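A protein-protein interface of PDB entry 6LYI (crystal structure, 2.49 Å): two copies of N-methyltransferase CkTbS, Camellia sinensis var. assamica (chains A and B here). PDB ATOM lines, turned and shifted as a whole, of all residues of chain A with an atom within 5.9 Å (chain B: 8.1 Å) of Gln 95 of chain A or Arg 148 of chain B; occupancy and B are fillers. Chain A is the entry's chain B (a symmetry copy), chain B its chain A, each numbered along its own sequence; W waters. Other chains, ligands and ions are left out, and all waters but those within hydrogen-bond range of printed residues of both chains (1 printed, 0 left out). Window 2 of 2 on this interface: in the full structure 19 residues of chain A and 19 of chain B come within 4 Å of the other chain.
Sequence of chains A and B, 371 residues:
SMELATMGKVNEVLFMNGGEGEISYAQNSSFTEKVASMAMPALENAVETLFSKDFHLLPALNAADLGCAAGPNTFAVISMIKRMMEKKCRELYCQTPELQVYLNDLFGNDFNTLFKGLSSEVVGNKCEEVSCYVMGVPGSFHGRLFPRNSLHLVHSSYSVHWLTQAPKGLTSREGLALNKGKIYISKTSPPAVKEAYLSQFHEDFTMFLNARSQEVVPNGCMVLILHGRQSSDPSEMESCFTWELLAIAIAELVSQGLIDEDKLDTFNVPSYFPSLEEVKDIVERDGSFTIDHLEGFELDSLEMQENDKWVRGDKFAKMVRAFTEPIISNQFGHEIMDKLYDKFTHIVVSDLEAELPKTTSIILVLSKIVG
The guanidinium group (NH2) of Arg 144 of chain B is in salt-bridge range of the side-chain carboxylate (OE2) of Glu 98 of chain A, at 2.9 Å.
The side-chain hydroxyl (OH) of Tyr 133 of chain A is in hydrogen-bond range of the guanidinium group (NH2) of Arg 144 of chain B (3.1 Å).
The guanidinium group (NH2) of Arg 148 of chain B lies within hydrogen-bond range of the backbone carbonyl oxygen (O) of Thr 96 of chain A (2.6 Å).
The guanidinium group of Arg 148 of chain B lies within salt-bridge range of the side-chain carboxylate of Glu 98 of chain A.
The backbone carbonyl oxygen of Phe 146 of chain B lies within hydrogen-bond range of the guanidinium group of Arg 144 of chain B (2.6 Å).
The side-chain carboxylate of Glu 215 of chain B is in salt-bridge range of the guanidinium group of Arg 144 of chain B.
The backbone NH (N) of Leu 145 of chain B lies within hydrogen-bond range of the side-chain carboxylate (OE2) of Glu 215 of chain B, at 2.8 Å.
The backbone NH of Phe 146 of chain B sits at hydrogen-bond distance from the side-chain carboxylate of Glu 215 of chain B (3.0 Å).
The backbone carbonyl oxygen (O) of Pro 59 of chain A lies within hydrogen-bond range of the backbone NH (N) of Glu 98 of chain A, at 3.2 Å.
The side-chain carboxylate of Glu 98 of chain A lies within hydrogen-bond range of the side-chain hydroxyl of Tyr 133 of chain A (2.8 Å).
Among the printed residues, merely in contact across the chains: Gln 95 of chain A with Arg 148 of chain B (3.5 Å), Glu 98 of chain A with Pro 147 of chain B (3.2 Å), Tyr 133 of chain A with Leu 145 of chain B (3.5 Å), Tyr 133 of chain A with Phe 146 of chain B (3.4 Å) and Tyr 133 of chain A with Pro 147 of chain B (3.7 Å).
Of the printed residues of chain B, Gln 95 of chain A touches Arg 148.
Arg 148 of chain B touches just these residues of chain A: Gln 95, Thr 96 and Glu 98.
Printed residues of chain A within 4 Å of Pro 147 of chain B: Glu 98 (3.2 Å) and Tyr 133 (3.7 Å).
Of the printed residues of chain B, Tyr 133 of chain A touches Arg 144, Leu 145, Phe 146 and Pro 147.
Asn 149 of chain B touches none of the printed residues of chain A.
Pro 218 of chain B touches none of the printed residues of chain A.
The nearest printed residue of chain A that does not touch Arg 148 of chain B is Pro 97 of chain A (4.1 Å).
Printed residues of chain B that touch a printed residue of chain A: Arg 144, Leu 145, Phe 146, Pro 147 and Arg 148.
Hydrophobic or aromatic side chains of chain B that line the printed part of chain A: Pro 147.
Along chain B the printed residues that touch a printed residue of chain A span positions 144 to 148.
Of the 9 printed residues of chain A, 4 touch a printed residue of chain B.
Among the printed residues, 9 pairs touch across the chains.
Among the printed residues, Asp or Glu carboxylates within 4 Å of a Lys or Arg side-chain nitrogen of the other chain: Glu 98 of chain A with Arg 144 of chain B and Glu 98 of chain A with Arg 148 of chain B.
No position is printed for both chains.
Water W1 lies within hydrogen-bond range of OE1 of Glu 98 of chain A, O of Pro 59 of chain A and NH2 of Arg 148 of chain B.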
ATOM      1  N   PRO A  59      -9.778  -7.795 -14.883  1.00  0.00           N
ATOM      2  CA  PRO A  59     -10.003  -8.027 -13.450  1.00  0.00           C
ATOM      3  C   PRO A  59      -8.785  -7.608 -12.619  1.00  0.00           C
ATOM      4  O   PRO A  59      -8.931  -6.967 -11.577  1.00  0.00           O
ATOM      5  CB  PRO A  59     -10.239  -9.543 -13.369  1.00  0.00           C
ATOM      6  CG  PRO A  59     -10.632  -9.947 -14.744  1.00  0.00           C
ATOM      7  CD  PRO A  59      -9.872  -9.045 -15.657  1.00  0.00           C
ATOM      8  N   LEU A  92     -15.246   4.347 -12.582  1.00  0.00           N
ATOM      9  CA  LEU A  92     -15.820   3.161 -13.222  1.00  0.00           C
ATOM     10  C   LEU A  92     -16.836   2.434 -12.330  1.00  0.00           C
ATOM     11  O   LEU A  92     -16.625   2.289 -11.125  1.00  0.00           O
ATOM     12  CB  LEU A  92     -14.699   2.197 -13.637  1.00  0.00           C
ATOM     13  CG  LEU A  92     -13.642   2.833 -14.546  1.00  0.00           C
ATOM     14  CD1 LEU A  92     -12.640   1.822 -14.997  1.00  0.00           C
ATOM     15  CD2 LEU A  92     -14.299   3.511 -15.744  1.00  0.00           C
ATOM     16  N   TYR A  93     -17.930   1.971 -12.934  1.00  0.00           N
ATOM     17  CA  TYR A  93     -19.005   1.327 -12.186  1.00  0.00           C
ATOM     18  C   TYR A  93     -18.656  -0.101 -11.789  1.00  0.00           C
ATOM     19  O   TYR A  93     -19.202  -0.640 -10.827  1.00  0.00           O
ATOM     20  CB  TYR A  93     -20.310   1.331 -12.990  1.00  0.00           C
ATOM     21  CG  TYR A  93     -20.992   2.676 -13.030  1.00  0.00           C
ATOM     22  CD1 TYR A  93     -20.633   3.629 -13.972  1.00  0.00           C
ATOM     23  CD2 TYR A  93     -21.998   2.996 -12.124  1.00  0.00           C
ATOM     24  CE1 TYR A  93     -21.253   4.863 -14.015  1.00  0.00           C
ATOM     25  CE2 TYR A  93     -22.620   4.227 -12.161  1.00  0.00           C
ATOM     26  CZ  TYR A  93     -22.243   5.157 -13.108  1.00  0.00           C
ATOM     27  OH  TYR A  93     -22.851   6.385 -13.150  1.00  0.00           O
ATOM     28  N   CYS A  94     -17.750  -0.720 -12.532  1.00  0.00           N
ATOM     29  CA  CYS A  94     -17.392  -2.106 -12.266  1.00  0.00           C
ATOM     30  C   CYS A  94     -16.611  -2.199 -10.958  1.00  0.00           C
ATOM     31  O   CYS A  94     -16.145  -1.189 -10.423  1.00  0.00           O
ATOM     32  CB  CYS A  94     -16.587  -2.698 -13.435  1.00  0.00           C
ATOM     33  SG  CYS A  94     -15.007  -1.895 -13.795  1.00  0.00           S
ATOM     34  N   GLN A  95     -16.509  -3.412 -10.429  1.00  0.00           N
ATOM     35  CA  GLN A  95     -15.709  -3.670  -9.241  1.00  0.00           C
ATOM     36  C   GLN A  95     -14.267  -3.263  -9.532  1.00  0.00           C
ATOM     37  O   GLN A  95     -13.788  -3.439 -10.655  1.00  0.00           O
ATOM     38  CB  GLN A  95     -15.806  -5.143  -8.850  1.00  0.00           C
ATOM     39  CG  GLN A  95     -15.297  -5.468  -7.466  1.00  0.00           C
ATOM     40  CD  GLN A  95     -15.565  -6.911  -7.095  1.00  0.00           C
ATOM     41  OE1 GLN A  95     -15.861  -7.739  -7.961  1.00  0.00           O
ATOM     42  NE2 GLN A  95     -15.469  -7.222  -5.806  1.00  0.00           N
ATOM     43  N   THR A  96     -13.580  -2.696  -8.545  1.00  0.00           N
ATOM     44  CA  THR A  96     -12.275  -2.101  -8.820  1.00  0.00           C
ATOM     45  C   THR A  96     -11.228  -3.166  -9.102  1.00  0.00           C
ATOM     46  O   THR A  96     -11.116  -4.147  -8.364  1.00  0.00           O
ATOM     47  CB  THR A  96     -11.781  -1.218  -7.666  1.00  0.00           C
ATOM     48  OG1 THR A  96     -12.771  -0.224  -7.365  1.00  0.00           O
ATOM     49  CG2 THR A  96     -10.464  -0.541  -8.051  1.00  0.00           C
ATOM     50  N   PRO A  97     -10.472  -2.983 -10.193  1.00  0.00           N
ATOM     51  CA  PRO A  97      -9.422  -3.945 -10.524  1.00  0.00           C
ATOM     52  C   PRO A  97      -8.357  -3.979  -9.447  1.00  0.00           C
ATOM     53  O   PRO A  97      -8.182  -3.026  -8.687  1.00  0.00           O
ATOM     54  CB  PRO A  97      -8.851  -3.418 -11.847  1.00  0.00           C
ATOM     55  CG  PRO A  97      -9.910  -2.538 -12.401  1.00  0.00           C
ATOM     56  CD  PRO A  97     -10.590  -1.928 -11.214  1.00  0.00           C
ATOM     57  N   GLU A  98      -7.656  -5.097  -9.385  1.00  0.00           N
ATOM     58  CA  GLU A  98      -6.559  -5.251  -8.463  1.00  0.00           C
ATOM     59  C   GLU A  98      -5.238  -5.229  -9.228  1.00  0.00           C
ATOM     60  O   GLU A  98      -5.214  -5.272 -10.452  1.00  0.00           O
ATOM     61  CB  GLU A  98      -6.740  -6.541  -7.674  1.00  0.00           C
ATOM     62  CG  GLU A  98      -8.123  -6.636  -7.038  1.00  0.00           C
ATOM     63  CD  GLU A  98      -8.432  -8.019  -6.488  1.00  0.00           C
ATOM     64  OE1 GLU A  98      -8.511  -8.967  -7.301  1.00  0.00           O
ATOM     65  OE2 GLU A  98      -8.593  -8.166  -5.252  1.00  0.00           O
ATOM     66  N   TYR A 133      -1.065  -6.836  -4.614  1.00  0.00           N
ATOM     67  CA  TYR A 133      -0.557  -8.104  -4.127  1.00  0.00           C
ATOM     68  C   TYR A 133       0.857  -8.302  -4.642  1.00  0.00           C
ATOM     69  O   TYR A 133       1.088  -8.343  -5.850  1.00  0.00           O
ATOM     70  CB  TYR A 133      -1.474  -9.240  -4.569  1.00  0.00           C
ATOM     71  CG  TYR A 133      -2.911  -9.025  -4.158  1.00  0.00           C
ATOM     72  CD1 TYR A 133      -3.297  -9.138  -2.832  1.00  0.00           C
ATOM     73  CD2 TYR A 133      -3.881  -8.701  -5.096  1.00  0.00           C
ATOM     74  CE1 TYR A 133      -4.604  -8.937  -2.448  1.00  0.00           C
ATOM     75  CE2 TYR A 133      -5.194  -8.504  -4.725  1.00  0.00           C
ATOM     76  CZ  TYR A 133      -5.552  -8.620  -3.395  1.00  0.00           C
ATOM     77  OH  TYR A 133      -6.864  -8.421  -3.002  1.00  0.00           O
ATOM     78  N   ARG B 144      -6.231 -11.474   2.616  1.00  0.00           N
ATOM     79  CA  ARG B 144      -6.069 -11.625   1.173  1.00  0.00           C
ATOM     80  C   ARG B 144      -4.600 -11.709   0.768  1.00  0.00           C
ATOM     81  O   ARG B 144      -3.744 -11.016   1.331  1.00  0.00           O
ATOM     82  CB  ARG B 144      -6.740 -10.460   0.435  1.00  0.00           C
ATOM     83  CG  ARG B 144      -8.262 -10.432   0.534  1.00  0.00           C
ATOM     84  CD  ARG B 144      -8.903 -11.535  -0.304  1.00  0.00           C
ATOM     85  NE  ARG B 144      -8.496 -11.471  -1.708  1.00  0.00           N
ATOM     86  CZ  ARG B 144      -9.101 -10.729  -2.634  1.00  0.00           C
ATOM     87  NH1 ARG B 144     -10.147  -9.981  -2.310  1.00  0.00           N
ATOM     88  NH2 ARG B 144      -8.661 -10.732  -3.888  1.00  0.00           N
ATOM     89  N   LEU B 145      -4.324 -12.547  -0.228  1.00  0.00           N
ATOM     90  CA  LEU B 145      -2.980 -12.703  -0.776  1.00  0.00           C
ATOM     91  C   LEU B 145      -2.964 -12.627  -2.305  1.00  0.00           C
ATOM     92  O   LEU B 145      -1.930 -12.358  -2.910  1.00  0.00           O
ATOM     93  CB  LEU B 145      -2.377 -14.032  -0.321  1.00  0.00           C
ATOM     94  CG  LEU B 145      -2.102 -14.158   1.178  1.00  0.00           C
ATOM     95  CD1 LEU B 145      -1.682 -15.580   1.528  1.00  0.00           C
ATOM     96  CD2 LEU B 145      -1.044 -13.150   1.612  1.00  0.00           C
ATOM     97  N   PHE B 146      -4.118 -12.859  -2.923  1.00  0.00           N
ATOM     98  CA  PHE B 146      -4.205 -13.031  -4.374  1.00  0.00           C
ATOM     99  C   PHE B 146      -5.352 -12.222  -4.969  1.00  0.00           C
ATOM    100  O   PHE B 146      -6.295 -11.862  -4.263  1.00  0.00           O
ATOM    101  CB  PHE B 146      -4.377 -14.519  -4.724  1.00  0.00           C
ATOM    102  CG  PHE B 146      -3.336 -15.406  -4.107  1.00  0.00           C
ATOM    103  CD1 PHE B 146      -2.067 -15.500  -4.662  1.00  0.00           C
ATOM    104  CD2 PHE B 146      -3.618 -16.139  -2.962  1.00  0.00           C
ATOM    105  CE1 PHE B 146      -1.097 -16.306  -4.084  1.00  0.00           C
ATOM    106  CE2 PHE B 146      -2.646 -16.950  -2.379  1.00  0.00           C
ATOM    107  CZ  PHE B 146      -1.385 -17.028  -2.936  1.00  0.00           C
ATOM    108  N   PRO B 147      -5.270 -11.922  -6.274  1.00  0.00           N
ATOM    109  CA  PRO B 147      -6.424 -11.312  -6.942  1.00  0.00           C
ATOM    110  C   PRO B 147      -7.656 -12.224  -6.899  1.00  0.00           C
ATOM    111  O   PRO B 147      -7.533 -13.426  -6.671  1.00  0.00           O
ATOM    112  CB  PRO B 147      -5.934 -11.117  -8.387  1.00  0.00           C
ATOM    113  CG  PRO B 147      -4.437 -11.026  -8.260  1.00  0.00           C
ATOM    114  CD  PRO B 147      -4.077 -11.966  -7.142  1.00  0.00           C
ATOM    115  N   ARG B 148      -8.834 -11.649  -7.110  1.00  0.00           N
ATOM    116  CA  ARG B 148     -10.062 -12.428  -7.188  1.00  0.00           C
ATOM    117  C   ARG B 148      -9.954 -13.494  -8.264  1.00  0.00           C
ATOM    118  O   ARG B 148      -9.315 -13.273  -9.293  1.00  0.00           O
ATOM    119  CB  ARG B 148     -11.263 -11.520  -7.481  1.00  0.00           C
ATOM    120  CG  ARG B 148     -11.594 -10.528  -6.356  1.00  0.00           C
ATOM    121  CD  ARG B 148     -12.790  -9.654  -6.705  1.00  0.00           C
ATOM    122  NE  ARG B 148     -12.484  -8.714  -7.778  1.00  0.00           N
ATOM    123  CZ  ARG B 148     -11.969  -7.505  -7.584  1.00  0.00           C
ATOM    124  NH1 ARG B 148     -11.705  -7.093  -6.348  1.00  0.00           N
ATOM    125  NH2 ARG B 148     -11.717  -6.712  -8.622  1.00  0.00           N
ATOM    126  N   ASN B 149     -10.566 -14.649  -8.022  1.00  0.00           N
ATOM    127  CA  ASN B 149     -10.706 -15.658  -9.060  1.00  0.00           C
ATOM    128  C   ASN B 149      -9.394 -16.043  -9.730  1.00  0.00           C
ATOM    129  O   ASN B 149      -9.301 -16.040 -10.955  1.00  0.00           O
ATOM    130  CB  ASN B 149     -11.677 -15.161 -10.127  1.00  0.00           C
ATOM    131  CG  ASN B 149     -13.025 -15.802 -10.013  1.00  0.00           C
ATOM    132  OD1 ASN B 149     -13.442 -16.558 -10.892  1.00  0.00           O
ATOM    133  ND2 ASN B 149     -13.706 -15.546  -8.907  1.00  0.00           N
ATOM    134  N   SER B 150      -8.379 -16.365  -8.938  1.00  0.00           N
ATOM    135  CA  SER B 150      -7.059 -16.604  -9.498  1.00  0.00           C
ATOM    136  C   SER B 150      -6.517 -17.975  -9.121  1.00  0.00           C
ATOM    137  O   SER B 150      -5.556 -18.452  -9.720  1.00  0.00           O
ATOM    138  CB  SER B 150      -6.093 -15.507  -9.048  1.00  0.00           C
ATOM    139  OG  SER B 150      -6.109 -15.368  -7.637  1.00  0.00           O
ATOM    140  N   LEU B 151      -7.139 -18.614  -8.137  1.00  0.00           N
ATOM    141  CA  LEU B 151      -6.649 -19.904  -7.671  1.00  0.00           C
ATOM    142  C   LEU B 151      -7.561 -21.041  -8.076  1.00  0.00           C
ATOM    143  O   LEU B 151      -8.776 -20.970  -7.901  1.00  0.00           O
ATOM    144  CB  LEU B 151      -6.485 -19.900  -6.154  1.00  0.00           C
ATOM    145  CG  LEU B 151      -5.527 -18.868  -5.574  1.00  0.00           C
ATOM    146  CD1 LEU B 151      -5.479 -19.014  -4.062  1.00  0.00           C
ATOM    147  CD2 LEU B 151      -4.147 -19.023  -6.183  1.00  0.00           C
ATOM    148  N   ALA B 211     -11.349 -14.954   2.914  1.00  0.00           N
ATOM    149  CA  ALA B 211     -10.309 -14.507   1.995  1.00  0.00           C
ATOM    150  C   ALA B 211     -10.224 -15.434   0.797  1.00  0.00           C
ATOM    151  O   ALA B 211     -10.232 -14.974  -0.342  1.00  0.00           O
ATOM    152  CB  ALA B 211      -8.947 -14.431   2.698  1.00  0.00           C
ATOM    153  N   ARG B 212     -10.145 -16.738   1.065  1.00  0.00           N
ATOM    154  CA  ARG B 212     -10.049 -17.747   0.012  1.00  0.00           C
ATOM    155  C   ARG B 212     -11.236 -17.719  -0.945  1.00  0.00           C
ATOM    156  O   ARG B 212     -11.093 -17.991  -2.138  1.00  0.00           O
ATOM    157  CB  ARG B 212      -9.924 -19.138   0.626  1.00  0.00           C
ATOM    158  CG  ARG B 212      -8.586 -19.401   1.307  1.00  0.00           C
ATOM    159  CD  ARG B 212      -7.446 -18.580   0.693  1.00  0.00           C
ATOM    160  NE  ARG B 212      -6.710 -17.937   1.783  1.00  0.00           N
ATOM    161  CZ  ARG B 212      -6.219 -16.707   1.736  1.00  0.00           C
ATOM    162  NH1 ARG B 212      -6.371 -15.977   0.649  1.00  0.00           N
ATOM    163  NH2 ARG B 212      -5.577 -16.215   2.774  1.00  0.00           N
ATOM    164  N   SER B 213     -12.409 -17.401  -0.408  1.00  0.00           N
ATOM    165  CA  SER B 213     -13.636 -17.333  -1.191  1.00  0.00           C
ATOM    166  C   SER B 213     -13.488 -16.374  -2.370  1.00  0.00           C
ATOM    167  O   SER B 213     -13.927 -16.662  -3.478  1.00  0.00           O
ATOM    168  CB  SER B 213     -14.805 -16.891  -0.302  1.00  0.00           C
ATOM    169  OG  SER B 213     -15.990 -16.727  -1.059  1.00  0.00           O
ATOM    170  N   GLN B 214     -12.870 -15.229  -2.107  1.00  0.00           N
ATOM    171  CA  GLN B 214     -12.608 -14.227  -3.122  1.00  0.00           C
ATOM    172  C   GLN B 214     -11.626 -14.718  -4.194  1.00  0.00           C
ATOM    173  O   GLN B 214     -11.711 -14.331  -5.361  1.00  0.00           O
ATOM    174  CB  GLN B 214     -12.052 -12.962  -2.463  1.00  0.00           C
ATOM    175  CG  GLN B 214     -13.020 -12.263  -1.556  1.00  0.00           C
ATOM    176  CD  GLN B 214     -14.312 -11.910  -2.269  1.00  0.00           C
ATOM    177  OE1 GLN B 214     -14.301 -11.431  -3.405  1.00  0.00           O
ATOM    178  NE2 GLN B 214     -15.435 -12.152  -1.607  1.00  0.00           N
ATOM    179  N   GLU B 215     -10.706 -15.587  -3.790  1.00  0.00           N
ATOM    180  CA  GLU B 215      -9.547 -15.915  -4.614  1.00  0.00           C
ATOM    181  C   GLU B 215      -9.713 -17.242  -5.316  1.00  0.00           C
ATOM    182  O   GLU B 215      -9.203 -17.436  -6.422  1.00  0.00           O
ATOM    183  CB  GLU B 215      -8.277 -15.926  -3.756  1.00  0.00           C
ATOM    184  CG  GLU B 215      -7.939 -14.565  -3.162  1.00  0.00           C
ATOM    185  CD  GLU B 215      -6.987 -14.652  -1.981  1.00  0.00           C
ATOM    186  OE1 GLU B 215      -6.602 -15.776  -1.608  1.00  0.00           O
ATOM    187  OE2 GLU B 215      -6.629 -13.596  -1.415  1.00  0.00           O
ATOM    188  N   VAL B 216     -10.419 -18.166  -4.677  1.00  0.00           N
ATOM    189  CA  VAL B 216     -10.600 -19.461  -5.296  1.00  0.00           C
ATOM    190  C   VAL B 216     -11.706 -19.391  -6.352  1.00  0.00           C
ATOM    191  O   VAL B 216     -12.839 -18.973  -6.101  1.00  0.00           O
ATOM    192  CB  VAL B 216     -10.897 -20.561  -4.259  1.00  0.00           C
ATOM    193  CG1 VAL B 216     -11.181 -21.889  -4.961  1.00  0.00           C
ATOM    194  CG2 VAL B 216      -9.715 -20.712  -3.328  1.00  0.00           C
ATOM    195  N   VAL B 217     -11.314 -19.792  -7.548  1.00  0.00           N
ATOM    196  CA  VAL B 217     -12.155 -19.840  -8.723  1.00  0.00           C
ATOM    197  C   VAL B 217     -13.360 -20.766  -8.491  1.00  0.00           C
ATOM    198  O   VAL B 217     -13.286 -21.701  -7.694  1.00  0.00           O
ATOM    199  CB  VAL B 217     -11.289 -20.303  -9.920  1.00  0.00           C
ATOM    200  CG1 VAL B 217     -11.793 -21.608 -10.520  1.00  0.00           C
ATOM    201  CG2 VAL B 217     -11.126 -19.186 -10.942  1.00  0.00           C
ATOM    202  N   PRO B 218     -14.496 -20.475  -9.143  1.00  0.00           N
ATOM    203  CA  PRO B 218     -15.694 -21.318  -9.017  1.00  0.00           C
ATOM    204  C   PRO B 218     -15.436 -22.799  -9.340  1.00  0.00           C
ATOM    205  O   PRO B 218     -14.930 -23.112 -10.412  1.00  0.00           O
ATOM    206  CB  PRO B 218     -16.658 -20.681 -10.018  1.00  0.00           C
ATOM    207  CG  PRO B 218     -16.293 -19.209  -9.937  1.00  0.00           C
ATOM    208  CD  PRO B 218     -14.786 -19.200  -9.823  1.00  0.00           C
HETATM  209  O   HOH W   1      -9.346  -8.882  -9.709  1.00  0.00           O
